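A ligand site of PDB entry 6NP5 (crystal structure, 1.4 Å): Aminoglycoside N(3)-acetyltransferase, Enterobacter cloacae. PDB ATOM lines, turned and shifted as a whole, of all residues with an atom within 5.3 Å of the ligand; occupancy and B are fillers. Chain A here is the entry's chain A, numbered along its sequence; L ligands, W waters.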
ATOM      1  N   PHE A  59      14.876  -4.957 -10.868  1.00  0.00           N
ATOM      2  CA  PHE A  59      14.703  -5.991 -11.888  1.00  0.00           C
ATOM      3  C   PHE A  59      13.324  -5.781 -12.505  1.00  0.00           C
ATOM      4  O   PHE A  59      12.301  -6.156 -11.919  1.00  0.00           O
ATOM      5  CB  PHE A  59      14.840  -7.364 -11.263  1.00  0.00           C
ATOM      6  CG  PHE A  59      14.499  -8.508 -12.200  1.00  0.00           C
ATOM      7  CD1 PHE A  59      14.723  -8.407 -13.572  1.00  0.00           C
ATOM      8  CD2 PHE A  59      13.936  -9.659 -11.716  1.00  0.00           C
ATOM      9  CE1 PHE A  59      14.381  -9.448 -14.418  1.00  0.00           C
ATOM     10  CE2 PHE A  59      13.613 -10.691 -12.551  1.00  0.00           C
ATOM     11  CZ  PHE A  59      13.835 -10.600 -13.892  1.00  0.00           C
ATOM     12  N   SER A  61      12.529  -6.449 -16.112  1.00  0.00           N
ATOM     13  CA  SER A  61      12.203  -7.381 -17.204  1.00  0.00           C
ATOM     14  C   SER A  61      11.457  -6.615 -18.292  1.00  0.00           C
ATOM     15  O   SER A  61      11.715  -5.428 -18.526  1.00  0.00           O
ATOM     16  CB  SER A  61      11.480  -8.608 -16.644  1.00  0.00           C
ATOM     17  OG  SER A  61      11.327  -9.600 -17.646  1.00  0.00           O
ATOM     18  N   SER A  65       8.411 -10.170 -23.067  1.00  0.00           N
ATOM     19  CA  SER A  65       9.521 -11.082 -23.284  1.00  0.00           C
ATOM     20  C   SER A  65       9.033 -12.410 -23.881  1.00  0.00           C
ATOM     21  O   SER A  65       8.151 -13.052 -23.296  1.00  0.00           O
ATOM     22  CB  SER A  65      10.228 -11.400 -21.984  1.00  0.00           C
ATOM     23  OG  SER A  65      11.234 -12.353 -22.268  1.00  0.00           O
ATOM     24  N   TYR A  67       9.945 -15.365 -23.673  1.00  0.00           N
ATOM     25  CA  TYR A  67      10.626 -16.430 -22.950  1.00  0.00           C
ATOM     26  C   TYR A  67       9.947 -17.772 -23.165  1.00  0.00           C
ATOM     27  O   TYR A  67      10.550 -18.701 -23.703  1.00  0.00           O
ATOM     28  CB  TYR A  67      10.677 -16.056 -21.469  1.00  0.00           C
ATOM     29  CG  TYR A  67      11.485 -17.009 -20.622  1.00  0.00           C
ATOM     30  CD1 TYR A  67      12.851 -16.798 -20.425  1.00  0.00           C
ATOM     31  CD2 TYR A  67      10.903 -18.084 -19.989  1.00  0.00           C
ATOM     32  CE1 TYR A  67      13.610 -17.639 -19.646  1.00  0.00           C
ATOM     33  CE2 TYR A  67      11.665 -18.950 -19.213  1.00  0.00           C
ATOM     34  CZ  TYR A  67      13.023 -18.720 -19.050  1.00  0.00           C
ATOM     35  OH  TYR A  67      13.814 -19.546 -18.259  1.00  0.00           O
ATOM     36  N   GLU A  68       8.675 -17.877 -22.773  1.00  0.00           N
ATOM     37  CA  GLU A  68       7.983 -19.159 -22.895  1.00  0.00           C
ATOM     38  C   GLU A  68       7.828 -19.576 -24.353  1.00  0.00           C
ATOM     39  O   GLU A  68       7.836 -20.775 -24.658  1.00  0.00           O
ATOM     40  CB  GLU A  68       6.604 -19.063 -22.244  1.00  0.00           C
ATOM     41  CG  GLU A  68       6.611 -18.976 -20.709  1.00  0.00           C
ATOM     42  CD  GLU A  68       6.614 -17.546 -20.179  1.00  0.00           C
ATOM     43  OE1 GLU A  68       6.938 -16.637 -20.946  1.00  0.00           O
ATOM     44  OE2 GLU A  68       6.263 -17.324 -19.012  1.00  0.00           O
ATOM     45  N   TYR A  95       7.705  -5.808 -16.843  1.00  0.00           N
ATOM     46  CA  TYR A  95       6.820  -6.957 -16.677  1.00  0.00           C
ATOM     47  C   TYR A  95       5.900  -6.760 -15.464  1.00  0.00           C
ATOM     48  O   TYR A  95       6.403  -6.647 -14.339  1.00  0.00           O
ATOM     49  CB  TYR A  95       7.639  -8.217 -16.482  1.00  0.00           C
ATOM     50  CG  TYR A  95       6.785  -9.455 -16.279  1.00  0.00           C
ATOM     51  CD1 TYR A  95       5.866  -9.854 -17.220  1.00  0.00           C
ATOM     52  CD2 TYR A  95       6.941 -10.251 -15.167  1.00  0.00           C
ATOM     53  CE1 TYR A  95       5.112 -11.001 -17.060  1.00  0.00           C
ATOM     54  CE2 TYR A  95       6.169 -11.411 -14.986  1.00  0.00           C
ATOM     55  CZ  TYR A  95       5.267 -11.778 -15.937  1.00  0.00           C
ATOM     56  OH  TYR A  95       4.504 -12.923 -15.774  1.00  0.00           O
ATOM     57  N   GLY A  97       4.177  -8.728 -13.652  1.00  0.00           N
ATOM     58  CA  GLY A  97       4.214  -9.778 -12.648  1.00  0.00           C
ATOM     59  C   GLY A  97       5.324  -9.652 -11.607  1.00  0.00           C
ATOM     60  O   GLY A  97       5.284 -10.389 -10.615  1.00  0.00           O
ATOM     61  N   PHE A  98       6.301  -8.764 -11.793  1.00  0.00           N
ATOM     62  CA  PHE A  98       7.376  -8.596 -10.814  1.00  0.00           C
ATOM     63  C   PHE A  98       7.159  -7.375  -9.942  1.00  0.00           C
ATOM     64  O   PHE A  98       8.046  -7.023  -9.134  1.00  0.00           O
ATOM     65  CB  PHE A  98       8.744  -8.559 -11.484  1.00  0.00           C
ATOM     66  CG  PHE A  98       9.095  -9.823 -12.236  1.00  0.00           C
ATOM     67  CD1 PHE A  98       8.506 -11.049 -11.936  1.00  0.00           C
ATOM     68  CD2 PHE A  98      10.046  -9.782 -13.237  1.00  0.00           C
ATOM     69  CE1 PHE A  98       8.863 -12.204 -12.643  1.00  0.00           C
ATOM     70  CE2 PHE A  98      10.384 -10.894 -13.941  1.00  0.00           C
ATOM     71  CZ  PHE A  98       9.793 -12.115 -13.649  1.00  0.00           C
ATOM     72  N   ASP A 118      15.006 -10.138 -21.222  1.00  0.00           N
ATOM     73  CA  ASP A 118      14.263 -10.912 -20.231  1.00  0.00           C
ATOM     74  C   ASP A 118      14.680 -10.541 -18.811  1.00  0.00           C
ATOM     75  O   ASP A 118      13.843 -10.508 -17.888  1.00  0.00           O
ATOM     76  CB  ASP A 118      14.432 -12.422 -20.484  1.00  0.00           C
ATOM     77  CG  ASP A 118      13.469 -13.234 -19.660  1.00  0.00           C
ATOM     78  OD1 ASP A 118      12.241 -13.215 -19.939  1.00  0.00           O
ATOM     79  OD2 ASP A 118      13.969 -13.863 -18.710  1.00  0.00           O
ATOM     80  N   TYR A 141      21.782 -13.094 -14.436  1.00  0.00           N
ATOM     81  CA  TYR A 141      21.869 -12.730 -13.026  1.00  0.00           C
ATOM     82  C   TYR A 141      23.233 -13.011 -12.421  1.00  0.00           C
ATOM     83  O   TYR A 141      23.438 -12.751 -11.231  1.00  0.00           O
ATOM     84  CB  TYR A 141      20.778 -13.413 -12.173  1.00  0.00           C
ATOM     85  CG  TYR A 141      19.425 -13.276 -12.812  1.00  0.00           C
ATOM     86  CD1 TYR A 141      18.726 -12.065 -12.830  1.00  0.00           C
ATOM     87  CD2 TYR A 141      18.894 -14.330 -13.531  1.00  0.00           C
ATOM     88  CE1 TYR A 141      17.542 -11.941 -13.513  1.00  0.00           C
ATOM     89  CE2 TYR A 141      17.666 -14.212 -14.208  1.00  0.00           C
ATOM     90  CZ  TYR A 141      17.015 -13.005 -14.215  1.00  0.00           C
ATOM     91  OH  TYR A 141      15.826 -12.837 -14.885  1.00  0.00           O
ATOM     92  N   ASP A 165      10.962 -15.478  -1.483  1.00  0.00           N
ATOM     93  CA  ASP A 165      11.129 -15.873  -2.875  1.00  0.00           C
ATOM     94  C   ASP A 165      11.462 -14.702  -3.793  1.00  0.00           C
ATOM     95  O   ASP A 165      11.899 -14.945  -4.922  1.00  0.00           O
ATOM     96  CB  ASP A 165       9.835 -16.486  -3.348  1.00  0.00           C
ATOM     97  CG  ASP A 165       8.686 -15.499  -3.291  1.00  0.00           C
ATOM     98  OD1 ASP A 165       8.290 -15.085  -2.162  1.00  0.00           O
ATOM     99  OD2 ASP A 165       8.230 -15.073  -4.371  1.00  0.00           O
ATOM    100  N   HIS A 171      19.802 -15.285  -7.383  1.00  0.00           N
ATOM    101  CA  HIS A 171      20.110 -16.002  -8.619  1.00  0.00           C
ATOM    102  C   HIS A 171      21.591 -15.916  -8.976  1.00  0.00           C
ATOM    103  O   HIS A 171      22.090 -16.798  -9.674  1.00  0.00           O
ATOM    104  CB  HIS A 171      19.213 -15.523  -9.756  1.00  0.00           C
ATOM    105  CG  HIS A 171      17.763 -15.833  -9.548  1.00  0.00           C
ATOM    106  ND1 HIS A 171      17.281 -17.106  -9.366  1.00  0.00           N
ATOM    107  CD2 HIS A 171      16.674 -15.035  -9.559  1.00  0.00           C
ATOM    108  CE1 HIS A 171      15.975 -17.078  -9.219  1.00  0.00           C
ATOM    109  NE2 HIS A 171      15.580 -15.833  -9.344  1.00  0.00           N
ATOM    110  N   SER A 207      16.563 -19.858 -14.193  1.00  0.00           N
ATOM    111  CA  SER A 207      16.184 -18.977 -13.096  1.00  0.00           C
ATOM    112  C   SER A 207      14.906 -19.425 -12.422  1.00  0.00           C
ATOM    113  O   SER A 207      14.493 -18.794 -11.450  1.00  0.00           O
ATOM    114  CB  SER A 207      16.054 -17.537 -13.582  1.00  0.00           C
ATOM    115  OG  SER A 207      14.954 -17.355 -14.438  1.00  0.00           O
ATOM    116  N   ASN A 208      14.293 -20.510 -12.896  1.00  0.00           N
ATOM    117  CA  ASN A 208      13.125 -21.082 -12.244  1.00  0.00           C
ATOM    118  C   ASN A 208      13.467 -22.276 -11.375  1.00  0.00           C
ATOM    119  O   ASN A 208      12.566 -22.993 -10.953  1.00  0.00           O
ATOM    120  CB  ASN A 208      12.046 -21.400 -13.256  1.00  0.00           C
ATOM    121  CG  ASN A 208      11.401 -20.158 -13.766  1.00  0.00           C
ATOM    122  OD1 ASN A 208      11.353 -19.863 -14.985  1.00  0.00           O
ATOM    123  ND2 ASN A 208      10.879 -19.403 -12.854  1.00  0.00           N
ATOM    124  N   GLY A 209      14.738 -22.482 -11.066  1.00  0.00           N
ATOM    125  CA  GLY A 209      15.143 -23.538 -10.172  1.00  0.00           C
ATOM    126  C   GLY A 209      16.469 -24.094 -10.629  1.00  0.00           C
ATOM    127  O   GLY A 209      16.552 -24.674 -11.718  1.00  0.00           O
ATOM    128  N   TYR A 214      14.419 -27.863  -6.929  1.00  0.00           N
ATOM    129  CA  TYR A 214      14.020 -26.480  -6.738  1.00  0.00           C
ATOM    130  C   TYR A 214      13.148 -25.933  -7.867  1.00  0.00           C
ATOM    131  O   TYR A 214      12.764 -24.754  -7.823  1.00  0.00           O
ATOM    132  CB  TYR A 214      15.272 -25.589  -6.592  1.00  0.00           C
ATOM    133  CG  TYR A 214      16.141 -25.990  -5.442  1.00  0.00           C
ATOM    134  CD1 TYR A 214      15.623 -26.091  -4.166  1.00  0.00           C
ATOM    135  CD2 TYR A 214      17.472 -26.283  -5.632  1.00  0.00           C
ATOM    136  CE1 TYR A 214      16.427 -26.517  -3.107  1.00  0.00           C
ATOM    137  CE2 TYR A 214      18.282 -26.670  -4.588  1.00  0.00           C
ATOM    138  CZ  TYR A 214      17.758 -26.775  -3.325  1.00  0.00           C
ATOM    139  OH  TYR A 214      18.559 -27.211  -2.294  1.00  0.00           O
ATOM    140  N   ALA A 216      10.021 -26.944  -9.168  1.00  0.00           N
ATOM    141  CA  ALA A 216       8.568 -27.031  -9.256  1.00  0.00           C
ATOM    142  C   ALA A 216       7.975 -25.668  -9.609  1.00  0.00           C
ATOM    143  O   ALA A 216       8.368 -24.649  -9.016  1.00  0.00           O
ATOM    144  CB  ALA A 216       7.982 -27.505  -7.921  1.00  0.00           C
ATOM    145  N   PRO A 217       7.019 -25.601 -10.548  1.00  0.00           N
ATOM    146  CA  PRO A 217       6.463 -24.286 -10.912  1.00  0.00           C
ATOM    147  C   PRO A 217       5.946 -23.496  -9.728  1.00  0.00           C
ATOM    148  O   PRO A 217       6.073 -22.264  -9.701  1.00  0.00           O
ATOM    149  CB  PRO A 217       5.348 -24.626 -11.916  1.00  0.00           C
ATOM    150  CG  PRO A 217       5.708 -25.965 -12.444  1.00  0.00           C
ATOM    151  CD  PRO A 217       6.373 -26.691 -11.306  1.00  0.00           C
ATOM    152  N   GLY A 219       7.126 -23.733  -6.666  1.00  0.00           N
ATOM    153  CA  GLY A 219       8.153 -23.615  -5.657  1.00  0.00           C
ATOM    154  C   GLY A 219       7.966 -24.632  -4.539  1.00  0.00           C
ATOM    155  O   GLY A 219       7.153 -25.554  -4.650  1.00  0.00           O
ATOM    156  N   ASP A 221      11.521 -22.601  -4.571  1.00  0.00           N
ATOM    157  CA  ASP A 221      12.789 -22.672  -5.241  1.00  0.00           C
ATOM    158  C   ASP A 221      13.926 -22.469  -4.246  1.00  0.00           C
ATOM    159  O   ASP A 221      13.717 -22.357  -3.030  1.00  0.00           O
ATOM    160  CB  ASP A 221      12.835 -21.699  -6.432  1.00  0.00           C
ATOM    161  CG  ASP A 221      13.021 -20.245  -6.022  1.00  0.00           C
ATOM    162  OD1 ASP A 221      12.767 -19.907  -4.872  1.00  0.00           O
ATOM    163  OD2 ASP A 221      13.387 -19.443  -6.914  1.00  0.00           O
ATOM    164  N   GLU A 224      13.942 -18.985  -2.440  1.00  0.00           N
ATOM    165  CA  GLU A 224      13.025 -18.897  -1.309  1.00  0.00           C
ATOM    166  C   GLU A 224      13.601 -19.632  -0.108  1.00  0.00           C
ATOM    167  O   GLU A 224      13.554 -19.134   1.022  1.00  0.00           O
ATOM    168  CB  GLU A 224      11.653 -19.458  -1.679  1.00  0.00           C
ATOM    169  CG  GLU A 224      10.691 -19.444  -0.519  1.00  0.00           C
ATOM    170  CD  GLU A 224       9.290 -19.906  -0.842  1.00  0.00           C
ATOM    171  OE1 GLU A 224       8.548 -20.227   0.113  1.00  0.00           O
ATOM    172  OE2 GLU A 224       8.897 -19.933  -2.038  1.00  0.00           O
HETATM  173  C1  LIG L   1       8.791 -16.833 -10.125  1.00  0.00           C
HETATM  174  C2  LIG L   1       7.893 -16.333  -9.009  1.00  0.00           C
HETATM  175  C3  LIG L   1       8.503 -16.538  -7.673  1.00  0.00           C
HETATM  176  C4  LIG L   1       8.816 -17.999  -7.448  1.00  0.00           C
HETATM  177  C5  LIG L   1       9.600 -18.570  -8.633  1.00  0.00           C
HETATM  178  C6  LIG L   1       9.693 -20.075  -8.566  1.00  0.00           C
HETATM  179  C7  LIG L   1      12.668 -15.004 -13.086  1.00  0.00           C
HETATM  180  C8  LIG L   1      11.592 -15.987 -13.541  1.00  0.00           C
HETATM  181  C9  LIG L   1      10.453 -16.058 -12.513  1.00  0.00           C
HETATM  182  C10 LIG L   1      10.959 -16.378 -11.099  1.00  0.00           C
HETATM  183  C11 LIG L   1      12.142 -15.497 -10.689  1.00  0.00           C
HETATM  184  C12 LIG L   1      13.249 -15.456 -11.748  1.00  0.00           C
HETATM  185  C13 LIG L   1      11.402 -16.270 -15.913  1.00  0.00           C
HETATM  186  C14 LIG L   1      11.368 -15.293 -17.083  1.00  0.00           C
HETATM  187  C15 LIG L   1       9.977 -14.749 -17.276  1.00  0.00           C
HETATM  188  C16 LIG L   1       9.042 -15.880 -17.483  1.00  0.00           C
HETATM  189  C17 LIG L   1       9.080 -16.849 -16.309  1.00  0.00           C
HETATM  190  C18 LIG L   1       8.157 -18.010 -16.431  1.00  0.00           C
HETATM  191  N1  LIG L   1      10.423 -20.560  -9.728  1.00  0.00           N
HETATM  192  N2  LIG L   1      12.670 -15.985  -9.404  1.00  0.00           N
HETATM  193  N3  LIG L   1      13.726 -14.908 -14.082  1.00  0.00           N
HETATM  194  N4  LIG L   1       9.938 -13.813 -18.455  1.00  0.00           N
HETATM  195  O1  LIG L   1       8.942 -18.278  -9.900  1.00  0.00           O
HETATM  196  O2  LIG L   1       7.576 -16.041  -6.657  1.00  0.00           O
HETATM  197  O3  LIG L   1       9.594 -18.229  -6.267  1.00  0.00           O
HETATM  198  O4  LIG L   1      10.007 -16.175 -10.060  1.00  0.00           O
HETATM  199  O5  LIG L   1       9.543 -17.066 -12.925  1.00  0.00           O
HETATM  200  O6  LIG L   1      11.049 -15.552 -14.769  1.00  0.00           O
HETATM  201  O7  LIG L   1      10.471 -17.358 -16.143  1.00  0.00           O
HETATM  202  O8  LIG L   1      12.257 -14.252 -16.752  1.00  0.00           O
HETATM  203  O9  LIG L   1       7.685 -15.415 -17.611  1.00  0.00           O
HETATM  204  O10 LIG L   1       8.401 -18.709 -17.586  1.00  0.00           O
HETATM  205  N5  LIG L   1       7.642 -14.870  -9.248  1.00  0.00           N
HETATM  206  O   HOH W   1       8.441 -21.192 -11.593  1.00  0.00           O
HETATM  207  O   HOH W   2      12.785 -18.950  -9.461  1.00  0.00           O
HETATM  208  O   HOH W   3      11.748 -14.071  -7.553  1.00  0.00           O
HETATM  209  O   HOH W   4       9.174 -21.541 -17.374  1.00  0.00           O
HETATM  210  O   HOH W   5      10.554 -23.258  -8.572  1.00  0.00           O
HETATM  211  O   HOH W   6       6.150 -15.040 -15.505  1.00  0.00           O
HETATM  212  O   HOH W   7       7.844 -13.845 -20.299  1.00  0.00           O
HETATM  213  O   HOH W   8      12.076 -17.101  -6.665  1.00  0.00           O
HETATM  214  O   HOH W   9       9.153 -11.381 -17.550  1.00  0.00           O
HETATM  215  O   HOH W  10       6.863 -16.400 -13.433  1.00  0.00           O
HETATM  216  O   HOH W  11       6.285 -14.614 -11.659  1.00  0.00           O
HETATM  217  O   HOH W  12       9.528 -12.758  -8.387  1.00  0.00           O
HETATM  218  O   HOH W  13       9.484 -20.342  -4.607  1.00  0.00           O
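A ring nitrogen (NE2) of His 171 sits at hydrogen-bond distance from a nitrogen (N2) of the ligand (2.9 Å).
An oxygen (O5) of the ligand is in hydrogen-bond range of the side-chain amide nitrogen of Asn 208, 2.7 Å away.
OG of Ser 207 sits at hydrogen-bond distance from N3 of the ligand (2.8 Å).
The side-chain carboxylate of Asp 165 sits at hydrogen-bond distance from an oxygen (O2) of the ligand (2.6 Å).
An oxygen (O9) of the ligand sits at hydrogen-bond distance from the side-chain carboxylate (OE2) of Glu 68, at 2.8 Å.
O of Asn 208 is in hydrogen-bond range of N1 of the ligand.
The side-chain hydroxyl (OH) of Tyr 141 lies within hydrogen-bond range of a nitrogen (N3) of the ligand (3.1 Å).
OD1 of Asp 118 lies within salt-bridge range of N4 of the ligand (2.8 Å).
The side-chain hydroxyl (OG) of Ser 65 is in hydrogen-bond range of the side-chain carboxylate (OD1) of Asp 118 (2.7 Å).
The side-chain hydroxyl of Ser 61 is in hydrogen-bond range of the backbone carbonyl oxygen of Asp 118, at 2.7 Å.
N of Glu 224 is in hydrogen-bond range of OD1 of Asp 221, at 2.9 Å.
Tyr 67 touches the ligand (CD2 to O10, 3.5 Å).
Phe 98 touches the ligand.
Asp 221 touches the ligand (OD1 to O3, 3.9 Å).
Of the 21 residues printed, 10 come within 4 Å of the ligand.
Water W6 lies within hydrogen-bond range of O9 of the ligand and OH of Tyr 95.
Water W13 lies within hydrogen-bond range of the side-chain carboxylate of Glu 224 (2.7 Å), an oxygen (O3) of the ligand (2.7 Å) and the backbone NH of Asp 221 (3.0 Å).
Water W9 lies within hydrogen-bond range of N4 of the ligand (2.7 Å) and OG of Ser 61 (2.8 Å).
Water W1 lies within hydrogen-bond range of a nitrogen (N1) of the ligand (2.8 Å), the backbone carbonyl oxygen of Pro 217 (3.2 Å) and the side-chain amide nitrogen of Asn 208 (3.3 Å).
Water W3 bridges O of Asp 165 and N2 of the ligand.
Water W2 lies within hydrogen-bond range of O of Ser 207, OD2 of Asp 221 and N1 of the ligand.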
